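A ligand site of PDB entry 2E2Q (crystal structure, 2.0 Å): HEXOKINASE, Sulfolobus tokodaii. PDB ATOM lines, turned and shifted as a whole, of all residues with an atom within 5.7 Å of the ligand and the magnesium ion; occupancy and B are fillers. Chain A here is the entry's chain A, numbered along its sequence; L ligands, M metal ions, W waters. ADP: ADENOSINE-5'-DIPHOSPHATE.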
ATOM      1  N   ASP A   8       5.437 -17.412  10.135  1.00  0.00           N
ATOM      2  CA  ASP A   8       4.036 -17.073   9.902  1.00  0.00           C
ATOM      3  C   ASP A   8       3.536 -18.207   9.010  1.00  0.00           C
ATOM      4  O   ASP A   8       3.833 -18.238   7.817  1.00  0.00           O
ATOM      5  CB  ASP A   8       3.933 -15.736   9.164  1.00  0.00           C
ATOM      6  CG  ASP A   8       2.497 -15.375   8.821  1.00  0.00           C
ATOM      7  OD1 ASP A   8       2.307 -14.488   7.953  1.00  0.00           O
ATOM      8  OD2 ASP A   8       1.565 -15.956   9.413  1.00  0.00           O
ATOM      9  N   ALA A   9       2.799 -19.150   9.585  1.00  0.00           N
ATOM     10  CA  ALA A   9       2.289 -20.308   8.854  1.00  0.00           C
ATOM     11  C   ALA A   9       0.849 -20.080   8.398  1.00  0.00           C
ATOM     12  O   ALA A   9      -0.078 -20.164   9.214  1.00  0.00           O
ATOM     13  CB  ALA A   9       2.390 -21.550   9.733  1.00  0.00           C
ATOM     14  N   GLY A  10       0.656 -19.811   7.107  1.00  0.00           N
ATOM     15  CA  GLY A  10      -0.685 -19.537   6.592  1.00  0.00           C
ATOM     16  C   GLY A  10      -1.356 -20.642   5.783  1.00  0.00           C
ATOM     17  O   GLY A  10      -0.930 -21.795   5.796  1.00  0.00           O
ATOM     18  N   GLY A  11      -2.434 -20.275   5.086  1.00  0.00           N
ATOM     19  CA  GLY A  11      -3.166 -21.253   4.281  1.00  0.00           C
ATOM     20  C   GLY A  11      -2.621 -21.411   2.869  1.00  0.00           C
ATOM     21  O   GLY A  11      -3.036 -22.315   2.152  1.00  0.00           O
ATOM     22  N   THR A  12      -1.700 -20.528   2.472  1.00  0.00           N
ATOM     23  CA  THR A  12      -1.096 -20.603   1.138  1.00  0.00           C
ATOM     24  C   THR A  12       0.415 -20.799   1.213  1.00  0.00           C
ATOM     25  O   THR A  12       0.987 -21.585   0.469  1.00  0.00           O
ATOM     26  CB  THR A  12      -1.387 -19.345   0.297  1.00  0.00           C
ATOM     27  OG1 THR A  12      -2.774 -19.314  -0.048  1.00  0.00           O
ATOM     28  CG2 THR A  12      -0.549 -19.372  -1.000  1.00  0.00           C
ATOM     29  N   LYS A  13       1.054 -20.082   2.118  1.00  0.00           N
ATOM     30  CA  LYS A  13       2.501 -20.187   2.276  1.00  0.00           C
ATOM     31  C   LYS A  13       2.879 -20.052   3.736  1.00  0.00           C
ATOM     32  O   LYS A  13       2.102 -19.571   4.559  1.00  0.00           O
ATOM     33  CB  LYS A  13       3.197 -19.077   1.488  1.00  0.00           C
ATOM     34  CG  LYS A  13       2.888 -17.699   2.026  1.00  0.00           C
ATOM     35  CD  LYS A  13       3.620 -16.589   1.283  1.00  0.00           C
ATOM     36  CE  LYS A  13       3.003 -16.305  -0.077  1.00  0.00           C
ATOM     37  NZ  LYS A  13       3.670 -15.138  -0.733  1.00  0.00           N
ATOM     38  N   THR A  14       4.096 -20.486   4.043  1.00  0.00           N
ATOM     39  CA  THR A  14       4.627 -20.368   5.380  1.00  0.00           C
ATOM     40  C   THR A  14       5.901 -19.561   5.178  1.00  0.00           C
ATOM     41  O   THR A  14       6.748 -19.897   4.350  1.00  0.00           O
ATOM     42  CB  THR A  14       4.942 -21.746   5.987  1.00  0.00           C
ATOM     43  OG1 THR A  14       3.718 -22.428   6.242  1.00  0.00           O
ATOM     44  CG2 THR A  14       5.709 -21.593   7.301  1.00  0.00           C
ATOM     45  N   LYS A  15       6.003 -18.470   5.932  1.00  0.00           N
ATOM     46  CA  LYS A  15       7.132 -17.560   5.848  1.00  0.00           C
ATOM     47  C   LYS A  15       7.888 -17.531   7.163  1.00  0.00           C
ATOM     48  O   LYS A  15       7.298 -17.351   8.229  1.00  0.00           O
ATOM     49  CB  LYS A  15       6.629 -16.147   5.523  1.00  0.00           C
ATOM     50  CG  LYS A  15       5.923 -16.031   4.177  1.00  0.00           C
ATOM     51  CD  LYS A  15       4.459 -15.569   4.300  1.00  0.00           C
ATOM     52  CE  LYS A  15       3.550 -16.636   4.898  1.00  0.00           C
ATOM     53  NZ  LYS A  15       2.091 -16.319   4.711  1.00  0.00           N
ATOM     54  N   ALA A  68      -2.095 -20.336  11.303  1.00  0.00           N
ATOM     55  CA  ALA A  68      -3.462 -20.251  10.811  1.00  0.00           C
ATOM     56  C   ALA A  68      -4.070 -21.627  11.053  1.00  0.00           C
ATOM     57  O   ALA A  68      -3.400 -22.642  10.870  1.00  0.00           O
ATOM     58  CB  ALA A  68      -3.449 -19.947   9.317  1.00  0.00           C
ATOM     59  N   ASP A  95      -2.155 -17.106  14.308  1.00  0.00           N
ATOM     60  CA  ASP A  95      -1.527 -16.178  13.376  1.00  0.00           C
ATOM     61  C   ASP A  95      -2.000 -14.733  13.536  1.00  0.00           C
ATOM     62  O   ASP A  95      -1.266 -13.809  13.192  1.00  0.00           O
ATOM     63  CB  ASP A  95      -1.683 -16.670  11.924  1.00  0.00           C
ATOM     64  CG  ASP A  95      -3.127 -16.632  11.404  1.00  0.00           C
ATOM     65  OD1 ASP A  95      -4.075 -16.776  12.192  1.00  0.00           O
ATOM     66  OD2 ASP A  95      -3.285 -16.468  10.183  1.00  0.00           O
ATOM     67  N   ILE A 113      -6.995  -9.842   9.299  1.00  0.00           N
ATOM     68  CA  ILE A 113      -6.200 -10.664   8.389  1.00  0.00           C
ATOM     69  C   ILE A 113      -7.118 -11.098   7.263  1.00  0.00           C
ATOM     70  O   ILE A 113      -8.212 -11.622   7.498  1.00  0.00           O
ATOM     71  CB  ILE A 113      -5.639 -11.953   9.034  1.00  0.00           C
ATOM     72  CG1 ILE A 113      -4.559 -11.600  10.067  1.00  0.00           C
ATOM     73  CG2 ILE A 113      -5.055 -12.869   7.956  1.00  0.00           C
ATOM     74  CD1 ILE A 113      -3.947 -12.812  10.752  1.00  0.00           C
ATOM     75  N   ALA A 114      -6.687 -10.841   6.039  1.00  0.00           N
ATOM     76  CA  ALA A 114      -7.429 -11.230   4.869  1.00  0.00           C
ATOM     77  C   ALA A 114      -6.407 -11.906   3.962  1.00  0.00           C
ATOM     78  O   ALA A 114      -5.733 -11.250   3.175  1.00  0.00           O
ATOM     79  CB  ALA A 114      -8.047  -9.988   4.181  1.00  0.00           C
ATOM     80  N   GLY A 115      -6.265 -13.212   4.129  1.00  0.00           N
ATOM     81  CA  GLY A 115      -5.329 -13.994   3.329  1.00  0.00           C
ATOM     82  C   GLY A 115      -6.144 -15.130   2.741  1.00  0.00           C
ATOM     83  O   GLY A 115      -7.246 -14.901   2.255  1.00  0.00           O
ATOM     84  N   THR A 116      -5.616 -16.351   2.804  1.00  0.00           N
ATOM     85  CA  THR A 116      -6.338 -17.523   2.296  1.00  0.00           C
ATOM     86  C   THR A 116      -7.683 -17.556   3.015  1.00  0.00           C
ATOM     87  O   THR A 116      -8.723 -17.838   2.418  1.00  0.00           O
ATOM     88  CB  THR A 116      -5.566 -18.826   2.578  1.00  0.00           C
ATOM     89  OG1 THR A 116      -4.260 -18.754   2.006  1.00  0.00           O
ATOM     90  CG2 THR A 116      -6.303 -20.022   1.973  1.00  0.00           C
ATOM     91  N   GLY A 117      -7.637 -17.261   4.314  1.00  0.00           N
ATOM     92  CA  GLY A 117      -8.838 -17.194   5.112  1.00  0.00           C
ATOM     93  C   GLY A 117      -8.841 -15.808   5.730  1.00  0.00           C
ATOM     94  O   GLY A 117      -8.065 -14.953   5.315  1.00  0.00           O
ATOM     95  N   ALA A 144      -9.425 -14.644   0.534  1.00  0.00           N
ATOM     96  CA  ALA A 144      -9.088 -14.982  -0.848  1.00  0.00           C
ATOM     97  C   ALA A 144      -9.921 -16.195  -1.287  1.00  0.00           C
ATOM     98  O   ALA A 144     -10.349 -16.271  -2.435  1.00  0.00           O
ATOM     99  CB  ALA A 144      -7.604 -15.259  -0.982  1.00  0.00           C
ATOM    100  N   TYR A 145     -10.138 -17.147  -0.385  1.00  0.00           N
ATOM    101  CA  TYR A 145     -10.938 -18.304  -0.725  1.00  0.00           C
ATOM    102  C   TYR A 145     -12.394 -17.847  -0.986  1.00  0.00           C
ATOM    103  O   TYR A 145     -13.029 -18.318  -1.918  1.00  0.00           O
ATOM    104  CB  TYR A 145     -10.942 -19.333   0.422  1.00  0.00           C
ATOM    105  CG  TYR A 145     -11.906 -20.478   0.197  1.00  0.00           C
ATOM    106  CD1 TYR A 145     -11.483 -21.673  -0.362  1.00  0.00           C
ATOM    107  CD2 TYR A 145     -13.272 -20.337   0.502  1.00  0.00           C
ATOM    108  CE1 TYR A 145     -12.362 -22.700  -0.633  1.00  0.00           C
ATOM    109  CE2 TYR A 145     -14.174 -21.365   0.236  1.00  0.00           C
ATOM    110  CZ  TYR A 145     -13.717 -22.540  -0.333  1.00  0.00           C
ATOM    111  OH  TYR A 145     -14.582 -23.559  -0.618  1.00  0.00           O
ATOM    112  N   ASP A 196      -6.013 -23.625  -0.952  1.00  0.00           N
ATOM    113  CA  ASP A 196      -5.108 -22.628  -1.498  1.00  0.00           C
ATOM    114  C   ASP A 196      -5.323 -22.424  -2.991  1.00  0.00           C
ATOM    115  O   ASP A 196      -5.154 -21.315  -3.504  1.00  0.00           O
ATOM    116  CB  ASP A 196      -3.647 -22.988  -1.191  1.00  0.00           C
ATOM    117  CG  ASP A 196      -3.218 -24.331  -1.781  1.00  0.00           C
ATOM    118  OD1 ASP A 196      -4.080 -25.196  -2.038  1.00  0.00           O
ATOM    119  OD2 ASP A 196      -2.001 -24.523  -1.965  1.00  0.00           O
ATOM    120  N   ALA A 199      -8.413 -20.220  -3.432  1.00  0.00           N
ATOM    121  CA  ALA A 199      -8.032 -18.890  -2.999  1.00  0.00           C
ATOM    122  C   ALA A 199      -7.100 -18.192  -4.002  1.00  0.00           C
ATOM    123  O   ALA A 199      -7.139 -16.974  -4.115  1.00  0.00           O
ATOM    124  CB  ALA A 199      -7.371 -18.973  -1.618  1.00  0.00           C
ATOM    125  N   SER A 200      -6.307 -18.952  -4.755  1.00  0.00           N
ATOM    126  CA  SER A 200      -5.395 -18.346  -5.729  1.00  0.00           C
ATOM    127  C   SER A 200      -6.158 -17.559  -6.793  1.00  0.00           C
ATOM    128  O   SER A 200      -5.628 -16.623  -7.396  1.00  0.00           O
ATOM    129  CB  SER A 200      -4.537 -19.415  -6.428  1.00  0.00           C
ATOM    130  OG  SER A 200      -5.323 -20.240  -7.276  1.00  0.00           O
ATOM    131  N   ILE A 201      -7.407 -17.956  -7.030  1.00  0.00           N
ATOM    132  CA  ILE A 201      -8.260 -17.302  -8.014  1.00  0.00           C
ATOM    133  C   ILE A 201      -8.530 -15.836  -7.652  1.00  0.00           C
ATOM    134  O   ILE A 201      -8.894 -15.041  -8.522  1.00  0.00           O
ATOM    135  CB  ILE A 201      -9.595 -18.095  -8.152  1.00  0.00           C
ATOM    136  CG1 ILE A 201      -9.289 -19.487  -8.729  1.00  0.00           C
ATOM    137  CG2 ILE A 201     -10.584 -17.344  -9.040  1.00  0.00           C
ATOM    138  CD1 ILE A 201     -10.435 -20.465  -8.632  1.00  0.00           C
ATOM    139  N   ALA A 202      -8.363 -15.459  -6.391  1.00  0.00           N
ATOM    140  CA  ALA A 202      -8.585 -14.069  -5.976  1.00  0.00           C
ATOM    141  C   ALA A 202      -7.718 -13.101  -6.788  1.00  0.00           C
ATOM    142  O   ALA A 202      -8.136 -11.998  -7.115  1.00  0.00           O
ATOM    143  CB  ALA A 202      -8.307 -13.887  -4.481  1.00  0.00           C
ATOM    144  N   LYS A 203      -6.495 -13.538  -7.112  1.00  0.00           N
ATOM    145  CA  LYS A 203      -5.569 -12.721  -7.903  1.00  0.00           C
ATOM    146  C   LYS A 203      -6.188 -12.391  -9.259  1.00  0.00           C
ATOM    147  O   LYS A 203      -6.032 -11.279  -9.769  1.00  0.00           O
ATOM    148  CB  LYS A 203      -4.264 -13.478  -8.134  1.00  0.00           C
ATOM    149  CG  LYS A 203      -3.178 -13.168  -7.127  1.00  0.00           C
ATOM    150  CD  LYS A 203      -2.064 -12.329  -7.765  1.00  0.00           C
ATOM    151  CE  LYS A 203      -2.599 -11.046  -8.374  1.00  0.00           C
ATOM    152  NZ  LYS A 203      -1.533 -10.284  -9.083  1.00  0.00           N
ATOM    153  N   ASP A 206      -8.760  -9.721  -8.970  1.00  0.00           N
ATOM    154  CA  ASP A 206      -8.128  -8.415  -8.865  1.00  0.00           C
ATOM    155  C   ASP A 206      -7.702  -7.922 -10.246  1.00  0.00           C
ATOM    156  O   ASP A 206      -7.932  -6.765 -10.600  1.00  0.00           O
ATOM    157  CB  ASP A 206      -6.907  -8.505  -7.949  1.00  0.00           C
ATOM    158  CG  ASP A 206      -6.303  -7.140  -7.662  1.00  0.00           C
ATOM    159  OD1 ASP A 206      -7.060  -6.218  -7.271  1.00  0.00           O
ATOM    160  OD2 ASP A 206      -5.082  -6.991  -7.805  1.00  0.00           O
ATOM    161  N   LEU A 220     -15.114  -8.048  -4.982  1.00  0.00           N
ATOM    162  CA  LEU A 220     -14.143  -7.495  -4.050  1.00  0.00           C
ATOM    163  C   LEU A 220     -14.831  -6.596  -3.030  1.00  0.00           C
ATOM    164  O   LEU A 220     -14.558  -6.681  -1.835  1.00  0.00           O
ATOM    165  CB  LEU A 220     -13.064  -6.727  -4.825  1.00  0.00           C
ATOM    166  CG  LEU A 220     -12.174  -7.596  -5.706  1.00  0.00           C
ATOM    167  CD1 LEU A 220     -11.243  -6.707  -6.540  1.00  0.00           C
ATOM    168  CD2 LEU A 220     -11.355  -8.551  -4.824  1.00  0.00           C
ATOM    169  N   GLY A 247      -2.449  -9.127   5.123  1.00  0.00           N
ATOM    170  CA  GLY A 247      -2.845 -10.221   4.255  1.00  0.00           C
ATOM    171  C   GLY A 247      -2.773  -9.975   2.768  1.00  0.00           C
ATOM    172  O   GLY A 247      -2.810  -8.836   2.304  1.00  0.00           O
ATOM    173  N   GLY A 248      -2.703 -11.070   2.020  1.00  0.00           N
ATOM    174  CA  GLY A 248      -2.618 -11.012   0.568  1.00  0.00           C
ATOM    175  C   GLY A 248      -3.773 -10.296  -0.104  1.00  0.00           C
ATOM    176  O   GLY A 248      -3.585  -9.678  -1.156  1.00  0.00           O
ATOM    177  N   MET A 249      -4.972 -10.362   0.476  1.00  0.00           N
ATOM    178  CA  MET A 249      -6.128  -9.691  -0.127  1.00  0.00           C
ATOM    179  C   MET A 249      -5.920  -8.187  -0.211  1.00  0.00           C
ATOM    180  O   MET A 249      -6.432  -7.526  -1.123  1.00  0.00           O
ATOM    181  CB  MET A 249      -7.406  -9.960   0.677  1.00  0.00           C
ATOM    182  CG  MET A 249      -8.069 -11.301   0.398  1.00  0.00           C
ATOM    183  SD  MET A 249      -8.295 -11.669  -1.369  1.00  0.00           S
ATOM    184  CE  MET A 249      -9.239 -10.289  -1.917  1.00  0.00           C
ATOM    185  N   ARG A 251      -3.447  -6.737  -1.111  1.00  0.00           N
ATOM    186  CA  ARG A 251      -2.558  -6.428  -2.221  1.00  0.00           C
ATOM    187  C   ARG A 251      -3.434  -5.942  -3.371  1.00  0.00           C
ATOM    188  O   ARG A 251      -2.954  -5.383  -4.361  1.00  0.00           O
ATOM    189  CB  ARG A 251      -1.737  -7.650  -2.622  1.00  0.00           C
ATOM    190  CG  ARG A 251      -0.573  -7.935  -1.676  1.00  0.00           C
ATOM    191  CD  ARG A 251       0.602  -8.572  -2.393  1.00  0.00           C
ATOM    192  NE  ARG A 251       0.659 -10.020  -2.187  1.00  0.00           N
ATOM    193  CZ  ARG A 251       1.513 -10.823  -2.822  1.00  0.00           C
ATOM    194  NH1 ARG A 251       1.504 -12.135  -2.571  1.00  0.00           N
ATOM    195  NH2 ARG A 251       2.371 -10.328  -3.706  1.00  0.00           N
ATOM    196  N   SER A 252      -4.740  -6.177  -3.239  1.00  0.00           N
ATOM    197  CA  SER A 252      -5.700  -5.714  -4.234  1.00  0.00           C
ATOM    198  C   SER A 252      -5.996  -4.264  -3.874  1.00  0.00           C
ATOM    199  O   SER A 252      -6.528  -3.991  -2.792  1.00  0.00           O
ATOM    200  CB  SER A 252      -6.991  -6.522  -4.173  1.00  0.00           C
ATOM    201  OG  SER A 252      -8.020  -5.896  -4.919  1.00  0.00           O
HETATM  202  PB  ADP L   1      -1.825 -16.992   4.009  1.00  0.00           P
HETATM  203  O1B ADP L   1      -3.086 -17.743   4.283  1.00  0.00           O
HETATM  204  O2B ADP L   1      -1.328 -16.202   5.181  1.00  0.00           O
HETATM  205  O3B ADP L   1      -0.722 -17.926   3.393  1.00  0.00           O
HETATM  206  PA  ADP L   1      -1.478 -14.648   2.334  1.00  0.00           P
HETATM  207  O1A ADP L   1      -1.747 -13.492   3.259  1.00  0.00           O
HETATM  208  O2A ADP L   1      -0.032 -14.962   2.079  1.00  0.00           O
HETATM  209  O3A ADP L   1      -2.226 -15.912   2.887  1.00  0.00           O
HETATM  210  O5' ADP L   1      -2.333 -14.247   1.048  1.00  0.00           O
HETATM  211  C5' ADP L   1      -2.217 -14.969  -0.221  1.00  0.00           C
HETATM  212  C4' ADP L   1      -3.554 -15.012  -0.947  1.00  0.00           C
HETATM  213  O4' ADP L   1      -4.010 -13.689  -1.371  1.00  0.00           O
HETATM  214  C3' ADP L   1      -3.686 -15.914  -2.198  1.00  0.00           C
HETATM  215  O3' ADP L   1      -4.797 -16.797  -1.957  1.00  0.00           O
HETATM  216  C2' ADP L   1      -3.888 -14.939  -3.377  1.00  0.00           C
HETATM  217  O2' ADP L   1      -4.899 -15.341  -4.313  1.00  0.00           O
HETATM  218  C1' ADP L   1      -4.299 -13.607  -2.748  1.00  0.00           C
HETATM  219  N9  ADP L   1      -3.684 -12.425  -3.426  1.00  0.00           N
HETATM  220  C8  ADP L   1      -2.378 -12.111  -3.602  1.00  0.00           C
HETATM  221  N7  ADP L   1      -2.201 -10.955  -4.278  1.00  0.00           N
HETATM  222  C5  ADP L   1      -3.465 -10.536  -4.531  1.00  0.00           C
HETATM  223  C6  ADP L   1      -3.977  -9.359  -5.232  1.00  0.00           C
HETATM  224  N6  ADP L   1      -3.256  -8.436  -5.780  1.00  0.00           N
HETATM  225  N1  ADP L   1      -5.362  -9.285  -5.284  1.00  0.00           N
HETATM  226  C2  ADP L   1      -6.201 -10.242  -4.717  1.00  0.00           C
HETATM  227  N3  ADP L   1      -5.754 -11.320  -4.080  1.00  0.00           N
HETATM  228  C4  ADP L   1      -4.395 -11.421  -4.008  1.00  0.00           C
HETATM  229 MG    MG M   1      -1.551 -15.275   6.936  1.00  0.00          MG
HETATM  230  O   HOH W   1      -0.369 -15.383  -3.105  1.00  0.00           O
HETATM  231  O   HOH W   2      -2.647 -13.817   5.747  1.00  0.00           O
HETATM  232  O   HOH W   3      -3.460 -16.094   7.634  1.00  0.00           O
HETATM  233  O   HOH W   4       0.428 -14.477   6.474  1.00  0.00           O
HETATM  234  O   HOH W   5      -1.773 -13.933   8.546  1.00  0.00           O
HETATM  235  O   HOH W   6      -0.621 -16.546   8.337  1.00  0.00           O
HETATM  236  O   HOH W   7       0.435 -12.606   4.621  1.00  0.00           O
HETATM  237  O   HOH W   8      -5.155 -17.494   5.855  1.00  0.00           O
HETATM  238  O   HOH W   9      -0.247 -10.343  -5.873  1.00  0.00           O
HETATM  239  O   HOH W  10      -3.729 -19.182  -2.605  1.00  0.00           O
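An oxygen (O3B) of the ligand is in hydrogen-bond range of the backbone NH (N) of Thr 12. The side-chain amino group (NZ) of Lys 15 lies within salt-bridge range of an oxygen (O3B) of the ligand. N of Lys 13 is in hydrogen-bond range of O3B of the ligand, at 3.1 Å. The backbone carbonyl oxygen of Arg 251 sits at hydrogen-bond distance from a nitrogen (N6) of the ligand (3.4 Å). O2' of the ligand is in hydrogen-bond range of O of Ala 199 (2.8 Å). An oxygen (O1B) of the ligand is in hydrogen-bond range of the backbone NH (N) of Gly 11 (2.7 Å). N of Gly 248 is in hydrogen-bond range of O1A of the ligand (2.9 Å). The backbone carbonyl oxygen of Ser 200 lies close to an oxygen (O2') of the ligand, 3.4 Å away. The backbone NH (N) of Thr 116 sits close to an oxygen (O1B) of the ligand (3.2 Å). A nitrogen (N6) of the ligand lies within hydrogen-bond range of the side-chain carboxylate of Asp 206, 3.1 Å away. The side-chain hydroxyl of Thr 116 lies within hydrogen-bond range of an oxygen (O1B) of the ligand, at 2.8 Å.
The backbone NH (N) of Gly 248 lies within hydrogen-bond range of the backbone carbonyl oxygen (O) of Ala 114 (3.2 Å). The backbone NH (N) of Ala 144 is in hydrogen-bond range of the backbone carbonyl oxygen (O) of Gly 115, 2.8 Å away. The backbone NH (N) of Met 249 lies within hydrogen-bond range of the backbone carbonyl oxygen (O) of Ala 114. The side-chain hydroxyl (OG) of Ser 252 lies within hydrogen-bond range of the side-chain carboxylate (OD1) of Asp 206 (2.6 Å). The side-chain carboxylate (OD1) of Asp 8 lies within salt-bridge range of the side-chain amino group (NZ) of Lys 15. The backbone carbonyl oxygen (O) of Thr 116 sits at hydrogen-bond distance from the backbone NH (N) of Tyr 145 (3.2 Å). O of Lys 13 sits close to NZ of Lys 15 (3.3 Å). The side-chain hydroxyl of Thr 12 lies within hydrogen-bond range of the side-chain hydroxyl of Thr 116.
The side-chain sulfur (SD) of Met 249 sits close to a nitrogen (N3) of the ligand (3.7 Å). Residues that only touch the ligand: Gly 10 (3.6 Å), Gly 115 (3.6 Å), Ala 144 (3.3 Å), Ala 202 (3.5 Å), Lys 203 (3.7 Å), Gly 247 (3.6 Å) and Ser 252 (3.4 Å). Of the 30 residues printed, 18 come within 4 Å of the ligand. Along chain A the residues within 4 Å of the ligand span positions 10 to 252.
OD2 of Asp 95 touches the magnesium ion, at 3.9 Å. Of the 30 residues printed, 1 comes within 4 Å of the magnesium ion. The nearest printed residue that does not touch the magnesium ion is Asp 8 (4.04 Å).
The magnesium ion is bound by O2B of the ligand (2.0 Å), water W5 (2.1 Å), water W6 (2.1 Å), water W2 (2.2 Å), water W4 (2.2 Å) and water W3 (2.2 Å). The magnesium ion has six donor atoms within binding distance.
Water W6 bridges the side-chain carboxylate of Asp 8 (2.5 Å) and the side-chain carboxylate of Asp 95 (3.2 Å). Water W4 lies within hydrogen-bond range of NZ of Lys 15 (3.0 Å) and OD2 of Asp 8 (3.5 Å). Water W9 lies within hydrogen-bond range of N7 of the ligand (2.6 Å), NH2 of Arg 251 (3.4 Å) and NZ of Lys 203 (3.5 Å). Water W8 lies within hydrogen-bond range of O1B of the ligand, N of Gly 117 and N of Thr 116. Water W10 lies within hydrogen-bond range of an oxygen (O3') of the ligand (2.7 Å), the backbone carbonyl oxygen of Asp 196 (2.7 Å), the side-chain hydroxyl of Thr 12 (2.7 Å) and the backbone NH of Ser 200 (3.4 Å).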
